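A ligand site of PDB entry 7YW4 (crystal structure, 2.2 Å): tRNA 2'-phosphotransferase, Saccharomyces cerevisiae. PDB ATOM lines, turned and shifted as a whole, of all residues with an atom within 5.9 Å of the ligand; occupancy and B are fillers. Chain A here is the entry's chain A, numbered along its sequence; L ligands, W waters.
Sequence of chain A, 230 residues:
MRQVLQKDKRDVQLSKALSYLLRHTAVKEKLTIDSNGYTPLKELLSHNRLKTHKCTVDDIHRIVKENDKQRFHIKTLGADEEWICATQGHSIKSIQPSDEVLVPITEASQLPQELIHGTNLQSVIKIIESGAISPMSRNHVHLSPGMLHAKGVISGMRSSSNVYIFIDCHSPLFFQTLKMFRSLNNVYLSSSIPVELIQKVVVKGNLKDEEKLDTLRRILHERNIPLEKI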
ATOM      1  N   ILE A 116       1.600  24.881  18.729  1.00  0.00           N
ATOM      2  CA  ILE A 116       0.912  24.887  17.441  1.00  0.00           C
ATOM      3  C   ILE A 116       1.493  25.983  16.571  1.00  0.00           C
ATOM      4  O   ILE A 116       1.689  27.120  17.037  1.00  0.00           O
ATOM      5  CB  ILE A 116      -0.607  25.088  17.642  1.00  0.00           C
ATOM      6  CG1 ILE A 116      -1.184  23.914  18.424  1.00  0.00           C
ATOM      7  CG2 ILE A 116      -1.312  25.232  16.302  1.00  0.00           C
ATOM      8  CD1 ILE A 116      -1.992  24.329  19.642  1.00  0.00           C
ATOM      9  N   HIS A 117       1.761  25.669  15.307  1.00  0.00           N
ATOM     10  CA  HIS A 117       2.125  26.658  14.309  1.00  0.00           C
ATOM     11  C   HIS A 117       0.969  26.789  13.328  1.00  0.00           C
ATOM     12  O   HIS A 117       0.665  25.846  12.585  1.00  0.00           O
ATOM     13  CB  HIS A 117       3.405  26.287  13.568  1.00  0.00           C
ATOM     14  CG  HIS A 117       3.798  27.266  12.510  1.00  0.00           C
ATOM     15  ND1 HIS A 117       4.343  28.510  12.804  1.00  0.00           N
ATOM     16  CD2 HIS A 117       3.729  27.209  11.158  1.00  0.00           C
ATOM     17  CE1 HIS A 117       4.589  29.154  11.686  1.00  0.00           C
ATOM     18  NE2 HIS A 117       4.229  28.386  10.669  1.00  0.00           N
ATOM     19  N   GLY A 118       0.332  27.956  13.306  1.00  0.00           N
ATOM     20  CA  GLY A 118      -0.777  28.199  12.414  1.00  0.00           C
ATOM     21  C   GLY A 118      -0.299  28.678  11.051  1.00  0.00           C
ATOM     22  O   GLY A 118       0.657  29.452  10.956  1.00  0.00           O
ATOM     23  N   THR A 119      -0.965  28.209  10.017  1.00  0.00           N
ATOM     24  CA  THR A 119      -0.570  28.486   8.646  1.00  0.00           C
ATOM     25  C   THR A 119      -1.738  28.098   7.739  1.00  0.00           C
ATOM     26  O   THR A 119      -2.827  27.763   8.215  1.00  0.00           O
ATOM     27  CB  THR A 119       0.724  27.748   8.291  1.00  0.00           C
ATOM     28  OG1 THR A 119       1.190  28.186   7.012  1.00  0.00           O
ATOM     29  CG2 THR A 119       0.505  26.249   8.256  1.00  0.00           C
ATOM     30  N   ASN A 120      -1.512  28.157   6.424  1.00  0.00           N
ATOM     31  CA  ASN A 120      -2.501  27.799   5.421  1.00  0.00           C
ATOM     32  C   ASN A 120      -2.042  26.545   4.681  1.00  0.00           C
ATOM     33  O   ASN A 120      -0.948  26.023   4.900  1.00  0.00           O
ATOM     34  CB  ASN A 120      -2.755  28.963   4.462  1.00  0.00           C
ATOM     35  CG  ASN A 120      -1.484  29.451   3.777  1.00  0.00           C
ATOM     36  OD1 ASN A 120      -0.596  28.674   3.466  1.00  0.00           O
ATOM     37  ND2 ASN A 120      -1.405  30.749   3.571  1.00  0.00           N
ATOM     38  N   SER A 123       1.244  26.727   2.434  1.00  0.00           N
ATOM     39  CA  SER A 123       2.513  26.744   3.154  1.00  0.00           C
ATOM     40  C   SER A 123       2.847  25.386   3.743  1.00  0.00           C
ATOM     41  O   SER A 123       4.020  25.002   3.784  1.00  0.00           O
ATOM     42  CB  SER A 123       2.478  27.800   4.258  1.00  0.00           C
ATOM     43  OG  SER A 123       2.242  29.085   3.737  1.00  0.00           O
ATOM     44  N   LYS A 126       4.605  23.253   1.168  1.00  0.00           N
ATOM     45  CA  LYS A 126       5.976  23.731   1.062  1.00  0.00           C
ATOM     46  C   LYS A 126       6.788  23.353   2.303  1.00  0.00           C
ATOM     47  O   LYS A 126       7.961  22.999   2.195  1.00  0.00           O
ATOM     48  CB  LYS A 126       6.014  25.242   0.882  1.00  0.00           C
ATOM     49  CG  LYS A 126       5.023  25.815  -0.105  1.00  0.00           C
ATOM     50  CD  LYS A 126       5.713  26.359  -1.341  1.00  0.00           C
ATOM     51  CE  LYS A 126       5.198  27.745  -1.663  1.00  0.00           C
ATOM     52  NZ  LYS A 126       5.633  28.219  -3.010  1.00  0.00           N
ATOM     53  N   ILE A 127       6.165  23.434   3.477  1.00  0.00           N
ATOM     54  CA  ILE A 127       6.868  23.091   4.712  1.00  0.00           C
ATOM     55  C   ILE A 127       7.305  21.637   4.702  1.00  0.00           C
ATOM     56  O   ILE A 127       8.452  21.303   4.985  1.00  0.00           O
ATOM     57  CB  ILE A 127       5.991  23.405   5.936  1.00  0.00           C
ATOM     58  CG1 ILE A 127       5.975  24.910   6.220  1.00  0.00           C
ATOM     59  CG2 ILE A 127       6.470  22.639   7.151  1.00  0.00           C
ATOM     60  CD1 ILE A 127       5.013  25.304   7.318  1.00  0.00           C
ATOM     61  N   SER A 130      10.059  21.006   1.812  1.00  0.00           N
ATOM     62  CA  SER A 130      11.379  21.536   2.109  1.00  0.00           C
ATOM     63  C   SER A 130      11.978  20.955   3.376  1.00  0.00           C
ATOM     64  O   SER A 130      13.179  21.131   3.620  1.00  0.00           O
ATOM     65  CB  SER A 130      11.335  23.068   2.211  1.00  0.00           C
ATOM     66  OG  SER A 130      10.624  23.496   3.360  1.00  0.00           O
ATOM     67  N   GLY A 131      11.179  20.269   4.201  1.00  0.00           N
ATOM     68  CA  GLY A 131      11.700  19.528   5.316  1.00  0.00           C
ATOM     69  C   GLY A 131      11.753  20.250   6.646  1.00  0.00           C
ATOM     70  O   GLY A 131      12.128  19.631   7.649  1.00  0.00           O
ATOM     71  N   ALA A 132      11.370  21.525   6.699  1.00  0.00           N
ATOM     72  CA  ALA A 132      11.448  22.227   7.963  1.00  0.00           C
ATOM     73  C   ALA A 132      10.509  23.421   7.975  1.00  0.00           C
ATOM     74  O   ALA A 132      10.264  24.042   6.938  1.00  0.00           O
ATOM     75  CB  ALA A 132      12.874  22.708   8.246  1.00  0.00           C
ATOM     76  N   ILE A 133      10.026  23.749   9.164  1.00  0.00           N
ATOM     77  CA  ILE A 133       9.305  25.038   9.357  1.00  0.00           C
ATOM     78  C   ILE A 133      10.437  26.006   9.659  1.00  0.00           C
ATOM     79  O   ILE A 133      11.170  25.786  10.583  1.00  0.00           O
ATOM     80  CB  ILE A 133       8.215  24.982  10.438  1.00  0.00           C
ATOM     81  CG1 ILE A 133       7.289  23.783  10.288  1.00  0.00           C
ATOM     82  CG2 ILE A 133       7.461  26.301  10.499  1.00  0.00           C
ATOM     83  CD1 ILE A 133       6.382  23.593  11.466  1.00  0.00           C
ATOM     84  N   SER A 134      10.609  27.017   8.805  1.00  0.00           N
ATOM     85  CA  SER A 134      11.759  27.945   8.921  1.00  0.00           C
ATOM     86  C   SER A 134      11.298  29.318   9.389  1.00  0.00           C
ATOM     87  O   SER A 134      10.182  29.718   9.071  1.00  0.00           O
ATOM     88  CB  SER A 134      12.475  28.045   7.608  1.00  0.00           C
ATOM     89  OG  SER A 134      12.912  29.367   7.368  1.00  0.00           O
ATOM     90  N   PRO A 135      12.160  30.067  10.102  1.00  0.00           N
ATOM     91  CA  PRO A 135      11.799  31.392  10.605  1.00  0.00           C
ATOM     92  C   PRO A 135      11.422  32.399   9.517  1.00  0.00           C
ATOM     93  O   PRO A 135      10.682  33.300   9.799  1.00  0.00           O
ATOM     94  CB  PRO A 135      13.086  31.811  11.342  1.00  0.00           C
ATOM     95  CG  PRO A 135      13.721  30.520  11.731  1.00  0.00           C
ATOM     96  CD  PRO A 135      13.489  29.650  10.516  1.00  0.00           C
ATOM     97  N   MET A 136      11.965  32.228   8.311  1.00  0.00           N
ATOM     98  CA  MET A 136      11.646  33.120   7.163  1.00  0.00           C
ATOM     99  C   MET A 136      12.070  34.567   7.465  1.00  0.00           C
ATOM    100  O   MET A 136      13.233  34.766   7.816  1.00  0.00           O
ATOM    101  CB  MET A 136      10.163  33.057   6.811  1.00  0.00           C
ATOM    102  CG  MET A 136       9.729  31.711   6.275  1.00  0.00           C
ATOM    103  SD  MET A 136      10.975  30.965   5.199  1.00  0.00           S
ATOM    104  CE  MET A 136       9.938  29.918   4.178  1.00  0.00           C
ATOM    105  N   SER A 137      11.153  35.511   7.311  1.00  0.00           N
ATOM    106  CA  SER A 137      11.444  36.943   7.590  1.00  0.00           C
ATOM    107  C   SER A 137      11.934  37.119   9.031  1.00  0.00           C
ATOM    108  O   SER A 137      12.960  37.765   9.226  1.00  0.00           O
ATOM    109  CB  SER A 137      10.235  37.800   7.345  1.00  0.00           C
ATOM    110  OG  SER A 137       9.232  37.538   8.312  1.00  0.00           O
ATOM    111  N   ARG A 138      11.208  36.555   9.983  1.00  0.00           N
ATOM    112  CA  ARG A 138      11.562  36.724  11.406  1.00  0.00           C
ATOM    113  C   ARG A 138      12.804  35.905  11.744  1.00  0.00           C
ATOM    114  O   ARG A 138      13.268  35.170  10.870  1.00  0.00           O
ATOM    115  CB  ARG A 138      10.386  36.312  12.295  1.00  0.00           C
ATOM    116  CG  ARG A 138       9.231  37.291  12.276  1.00  0.00           C
ATOM    117  CD  ARG A 138       7.896  36.609  12.521  1.00  0.00           C
ATOM    118  NE  ARG A 138       6.887  37.075  11.600  1.00  0.00           N
ATOM    119  CZ  ARG A 138       6.030  38.060  11.860  1.00  0.00           C
ATOM    120  NH1 ARG A 138       6.059  38.683  13.021  1.00  0.00           N
ATOM    121  NH2 ARG A 138       5.138  38.415  10.943  1.00  0.00           N
ATOM    122  N   HIS A 140      12.813  33.803  14.280  1.00  0.00           N
ATOM    123  CA  HIS A 140      12.344  32.567  14.942  1.00  0.00           C
ATOM    124  C   HIS A 140      11.007  32.105  14.379  1.00  0.00           C
ATOM    125  O   HIS A 140      10.290  32.919  13.803  1.00  0.00           O
ATOM    126  CB  HIS A 140      12.257  32.778  16.458  1.00  0.00           C
ATOM    127  CG  HIS A 140      13.564  32.901  17.144  1.00  0.00           C
ATOM    128  ND1 HIS A 140      14.100  34.129  17.489  1.00  0.00           N
ATOM    129  CD2 HIS A 140      14.445  31.969  17.566  1.00  0.00           C
ATOM    130  CE1 HIS A 140      15.252  33.941  18.096  1.00  0.00           C
ATOM    131  NE2 HIS A 140      15.488  32.635  18.158  1.00  0.00           N
ATOM    132  N   HIS A 142       7.304  31.235  14.959  1.00  0.00           N
ATOM    133  CA  HIS A 142       6.332  31.638  16.005  1.00  0.00           C
ATOM    134  C   HIS A 142       5.371  30.475  16.270  1.00  0.00           C
ATOM    135  O   HIS A 142       4.853  29.914  15.307  1.00  0.00           O
ATOM    136  CB  HIS A 142       5.664  32.960  15.607  1.00  0.00           C
ATOM    137  CG  HIS A 142       6.589  34.129  15.654  1.00  0.00           C
ATOM    138  ND1 HIS A 142       6.167  35.383  16.038  1.00  0.00           N
ATOM    139  CD2 HIS A 142       7.898  34.236  15.389  1.00  0.00           C
ATOM    140  CE1 HIS A 142       7.184  36.213  15.993  1.00  0.00           C
ATOM    141  NE2 HIS A 142       8.256  35.533  15.605  1.00  0.00           N
ATOM    142  N   LEU A 143       5.157  30.166  17.541  1.00  0.00           N
ATOM    143  CA  LEU A 143       4.311  29.017  17.928  1.00  0.00           C
ATOM    144  C   LEU A 143       3.332  29.456  19.010  1.00  0.00           C
ATOM    145  O   LEU A 143       3.717  30.180  19.922  1.00  0.00           O
ATOM    146  CB  LEU A 143       5.216  27.895  18.427  1.00  0.00           C
ATOM    147  CG  LEU A 143       6.205  27.330  17.417  1.00  0.00           C
ATOM    148  CD1 LEU A 143       7.291  26.538  18.112  1.00  0.00           C
ATOM    149  CD2 LEU A 143       5.494  26.470  16.389  1.00  0.00           C
ATOM    150  N   SER A 144       2.087  29.005  18.884  1.00  0.00           N
ATOM    151  CA  SER A 144       1.040  29.364  19.854  1.00  0.00           C
ATOM    152  C   SER A 144       0.850  28.231  20.848  1.00  0.00           C
ATOM    153  O   SER A 144       0.698  27.081  20.427  1.00  0.00           O
ATOM    154  CB  SER A 144      -0.243  29.689  19.142  1.00  0.00           C
ATOM    155  OG  SER A 144      -1.294  29.845  20.064  1.00  0.00           O
ATOM    156  N   MET A 157      -2.562  33.389  16.828  1.00  0.00           N
ATOM    157  CA  MET A 157      -2.361  33.023  15.433  1.00  0.00           C
ATOM    158  C   MET A 157      -3.174  33.904  14.508  1.00  0.00           C
ATOM    159  O   MET A 157      -4.178  34.488  14.906  1.00  0.00           O
ATOM    160  CB  MET A 157      -2.742  31.566  15.189  1.00  0.00           C
ATOM    161  CG  MET A 157      -1.749  30.530  15.657  1.00  0.00           C
ATOM    162  SD  MET A 157      -2.465  28.892  15.498  1.00  0.00           S
ATOM    163  CE  MET A 157      -4.119  29.316  14.951  1.00  0.00           C
ATOM    164  N   ARG A 158      -2.736  33.990  13.246  1.00  0.00           N
ATOM    165  CA  ARG A 158      -3.475  34.746  12.250  1.00  0.00           C
ATOM    166  C   ARG A 158      -4.870  34.158  12.096  1.00  0.00           C
ATOM    167  O   ARG A 158      -5.045  32.939  12.044  1.00  0.00           O
ATOM    168  CB  ARG A 158      -2.739  34.740  10.913  1.00  0.00           C
ATOM    169  CG  ARG A 158      -1.721  35.871  10.762  1.00  0.00           C
ATOM    170  CD  ARG A 158      -2.357  37.231  11.035  1.00  0.00           C
ATOM    171  NE  ARG A 158      -1.896  37.797  12.300  1.00  0.00           N
ATOM    172  CZ  ARG A 158      -2.667  38.407  13.181  1.00  0.00           C
ATOM    173  NH1 ARG A 158      -3.968  38.570  12.970  1.00  0.00           N
ATOM    174  NH2 ARG A 158      -2.132  38.864  14.315  1.00  0.00           N
ATOM    175  N   SER A 161      -5.600  31.497   9.476  1.00  0.00           N
ATOM    176  CA  SER A 161      -4.834  30.233   9.545  1.00  0.00           C
ATOM    177  C   SER A 161      -5.787  29.033   9.616  1.00  0.00           C
ATOM    178  O   SER A 161      -6.450  28.882  10.633  1.00  0.00           O
ATOM    179  CB  SER A 161      -3.812  30.292  10.637  1.00  0.00           C
ATOM    180  OG  SER A 161      -2.866  31.318  10.406  1.00  0.00           O
ATOM    181  N   VAL A 187       4.244  33.693  23.917  1.00  0.00           N
ATOM    182  CA  VAL A 187       4.415  33.173  22.571  1.00  0.00           C
ATOM    183  C   VAL A 187       5.772  32.497  22.511  1.00  0.00           C
ATOM    184  O   VAL A 187       6.762  33.031  23.037  1.00  0.00           O
ATOM    185  CB  VAL A 187       4.301  34.277  21.489  1.00  0.00           C
ATOM    186  CG1 VAL A 187       4.820  33.771  20.153  1.00  0.00           C
ATOM    187  CG2 VAL A 187       2.853  34.725  21.357  1.00  0.00           C
ATOM    188  N   TYR A 188       5.822  31.333  21.889  1.00  0.00           N
ATOM    189  CA  TYR A 188       7.037  30.544  21.864  1.00  0.00           C
ATOM    190  C   TYR A 188       7.778  30.775  20.547  1.00  0.00           C
ATOM    191  O   TYR A 188       7.162  30.800  19.476  1.00  0.00           O
ATOM    192  CB  TYR A 188       6.717  29.065  22.065  1.00  0.00           C
ATOM    193  CG  TYR A 188       6.292  28.773  23.492  1.00  0.00           C
ATOM    194  CD1 TYR A 188       5.073  29.228  23.975  1.00  0.00           C
ATOM    195  CD2 TYR A 188       7.131  28.088  24.360  1.00  0.00           C
ATOM    196  CE1 TYR A 188       4.691  28.988  25.284  1.00  0.00           C
ATOM    197  CE2 TYR A 188       6.759  27.846  25.678  1.00  0.00           C
ATOM    198  CZ  TYR A 188       5.534  28.298  26.124  1.00  0.00           C
ATOM    199  OH  TYR A 188       5.151  28.058  27.433  1.00  0.00           O
HETATM  200  P1  LIG L   1       5.607  34.907   9.360  1.00  0.00           P
HETATM  201  O1  LIG L   1       7.058  35.101   9.621  1.00  0.00           O
HETATM  202  O2  LIG L   1       4.689  36.062   9.439  1.00  0.00           O
HETATM  203  O3  LIG L   1       5.400  34.210   7.941  1.00  0.00           O
HETATM  204  C1  LIG L   1       6.205  33.075   7.568  1.00  0.00           C
HETATM  205  C2  LIG L   1       5.321  32.101   6.846  1.00  0.00           C
HETATM  206  O4  LIG L   1       6.138  31.134   6.159  1.00  0.00           O
HETATM  207  C3  LIG L   1       4.369  31.297   7.741  1.00  0.00           C
HETATM  208  O5  LIG L   1       3.106  31.214   7.134  1.00  0.00           O
HETATM  209  C4  LIG L   1       5.031  29.917   7.800  1.00  0.00           C
HETATM  210  O6  LIG L   1       4.050  28.925   8.036  1.00  0.00           O
HETATM  211  C5  LIG L   1       5.636  29.844   6.406  1.00  0.00           C
HETATM  212  N1  LIG L   1       6.717  28.891   6.273  1.00  0.00           N
HETATM  213  C6  LIG L   1       7.515  28.428   7.281  1.00  0.00           C
HETATM  214  N2  LIG L   1       8.412  27.560   6.885  1.00  0.00           N
HETATM  215  C7  LIG L   1       8.190  27.453   5.528  1.00  0.00           C
HETATM  216  C8  LIG L   1       8.825  26.691   4.523  1.00  0.00           C
HETATM  217  N3  LIG L   1       9.831  25.863   4.750  1.00  0.00           N
HETATM  218  N4  LIG L   1       8.368  26.812   3.270  1.00  0.00           N
HETATM  219  N5  LIG L   1       6.684  28.407   3.890  1.00  0.00           N
HETATM  220  C9  LIG L   1       7.158  28.268   5.140  1.00  0.00           C
HETATM  221  O7  LIG L   1       5.064  33.799  10.360  1.00  0.00           O
HETATM  222  P2  LIG L   1       3.691  33.806  11.169  1.00  0.00           P
HETATM  223  O8  LIG L   1       3.812  32.918  12.355  1.00  0.00           O
HETATM  224  O9  LIG L   1       2.582  33.583  10.215  1.00  0.00           O
HETATM  225  O10 LIG L   1       3.645  35.325  11.648  1.00  0.00           O
HETATM  226  C10 LIG L   1       4.013  35.609  13.012  1.00  0.00           C
HETATM  227  C11 LIG L   1       2.963  36.498  13.628  1.00  0.00           C
HETATM  228  O11 LIG L   1       1.906  35.673  14.166  1.00  0.00           O
HETATM  229  C12 LIG L   1       3.459  37.324  14.828  1.00  0.00           C
HETATM  230  O12 LIG L   1       2.644  38.464  15.025  1.00  0.00           O
HETATM  231  O13 LIG L   1       3.270  36.865  17.239  1.00  0.00           O
HETATM  232  C13 LIG L   1       1.990  35.625  15.580  1.00  0.00           C
HETATM  233  C14 LIG L   1       2.022  33.184  15.117  1.00  0.00           C
HETATM  234  C15 LIG L   1       1.559  30.764  14.561  1.00  0.00           C
HETATM  235  O14 LIG L   1       0.904  29.795  14.924  1.00  0.00           O
HETATM  236  N6  LIG L   1       2.043  30.891  13.342  1.00  0.00           N
HETATM  237  C16 LIG L   1       1.943  31.604  16.899  1.00  0.00           C
HETATM  238  C17 LIG L   1       1.817  33.930  17.339  1.00  0.00           C
HETATM  239  O   HOH W   1       7.055  31.901  12.470  1.00  0.00           O
HETATM  240  O   HOH W   2       7.683  30.144  10.034  1.00  0.00           O
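SD of Met 157 lies close to N of Gly 118 (3.7 Å). O of His 142 sits at hydrogen-bond distance from ND1 of His 117 (2.9 Å). OG of Ser 130 sits at hydrogen-bond distance from O of Ile 127 (3.5 Å). O of Lys 126 lies within hydrogen-bond range of OG of Ser 130 (2.9 Å). The backbone carbonyl oxygen (O) of Ile 127 sits at hydrogen-bond distance from the backbone NH (N) of Ala 132 (3.4 Å). OG of Ser 134 lies within hydrogen-bond range of N of Met 136, at 3.2 Å. The backbone NH (N) of Ser 144 is in hydrogen-bond range of the backbone carbonyl oxygen (O) of Ile 116 (2.7 Å). O of Tyr 188 sits at hydrogen-bond distance from N of Leu 143, at 2.9 Å.
Water W1 bridges N of His 142 and O8 of the ligand.
O14 of the ligand lies close to O of Ile 116 (3.5 Å). O14 of the ligand sits close to SD of Met 157, 3.5 Å away. Merely in contact with the ligand: Lys 126 (3.7 Å), Ile 127 (3.4 Å), Ile 133 (3.6 Å), Met 136 (3.3 Å), Ser 137 (3.5 Å), Leu 143 (3.3 Å) and Ser 144 (3.3 Å). Hydrophobic or aromatic side chains within 4 Å of the ligand: His 117, Ile 127, Ile 133, Met 136, His 142 and Met 157.
The backbone NH (N) of Gly 118 is in hydrogen-bond range of an oxygen (O14) of the ligand, at 2.5 Å. N6 of the ligand sits at hydrogen-bond distance from O of Gly 118. An oxygen (O6) of the ligand is in hydrogen-bond range of a ring nitrogen (NE2) of His 117 (2.7 Å). NE of Arg 138 is in salt-bridge range of O1 of the ligand (2.8 Å). OG of Ser 130 lies within hydrogen-bond range of N3 of the ligand, at 2.9 Å. The backbone carbonyl oxygen of Ala 132 lies within hydrogen-bond range of a nitrogen (N3) of the ligand (2.9 Å). The backbone NH (N) of Ser 134 is in hydrogen-bond range of a nitrogen (N2) of the ligand (3.0 Å). An oxygen (O6) of the ligand sits at hydrogen-bond distance from the side-chain hydroxyl (OG1) of Thr 119 (3.1 Å). A ring nitrogen (ND1) of His 142 is in hydrogen-bond range of an oxygen (O13) of the ligand (3.5 Å).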
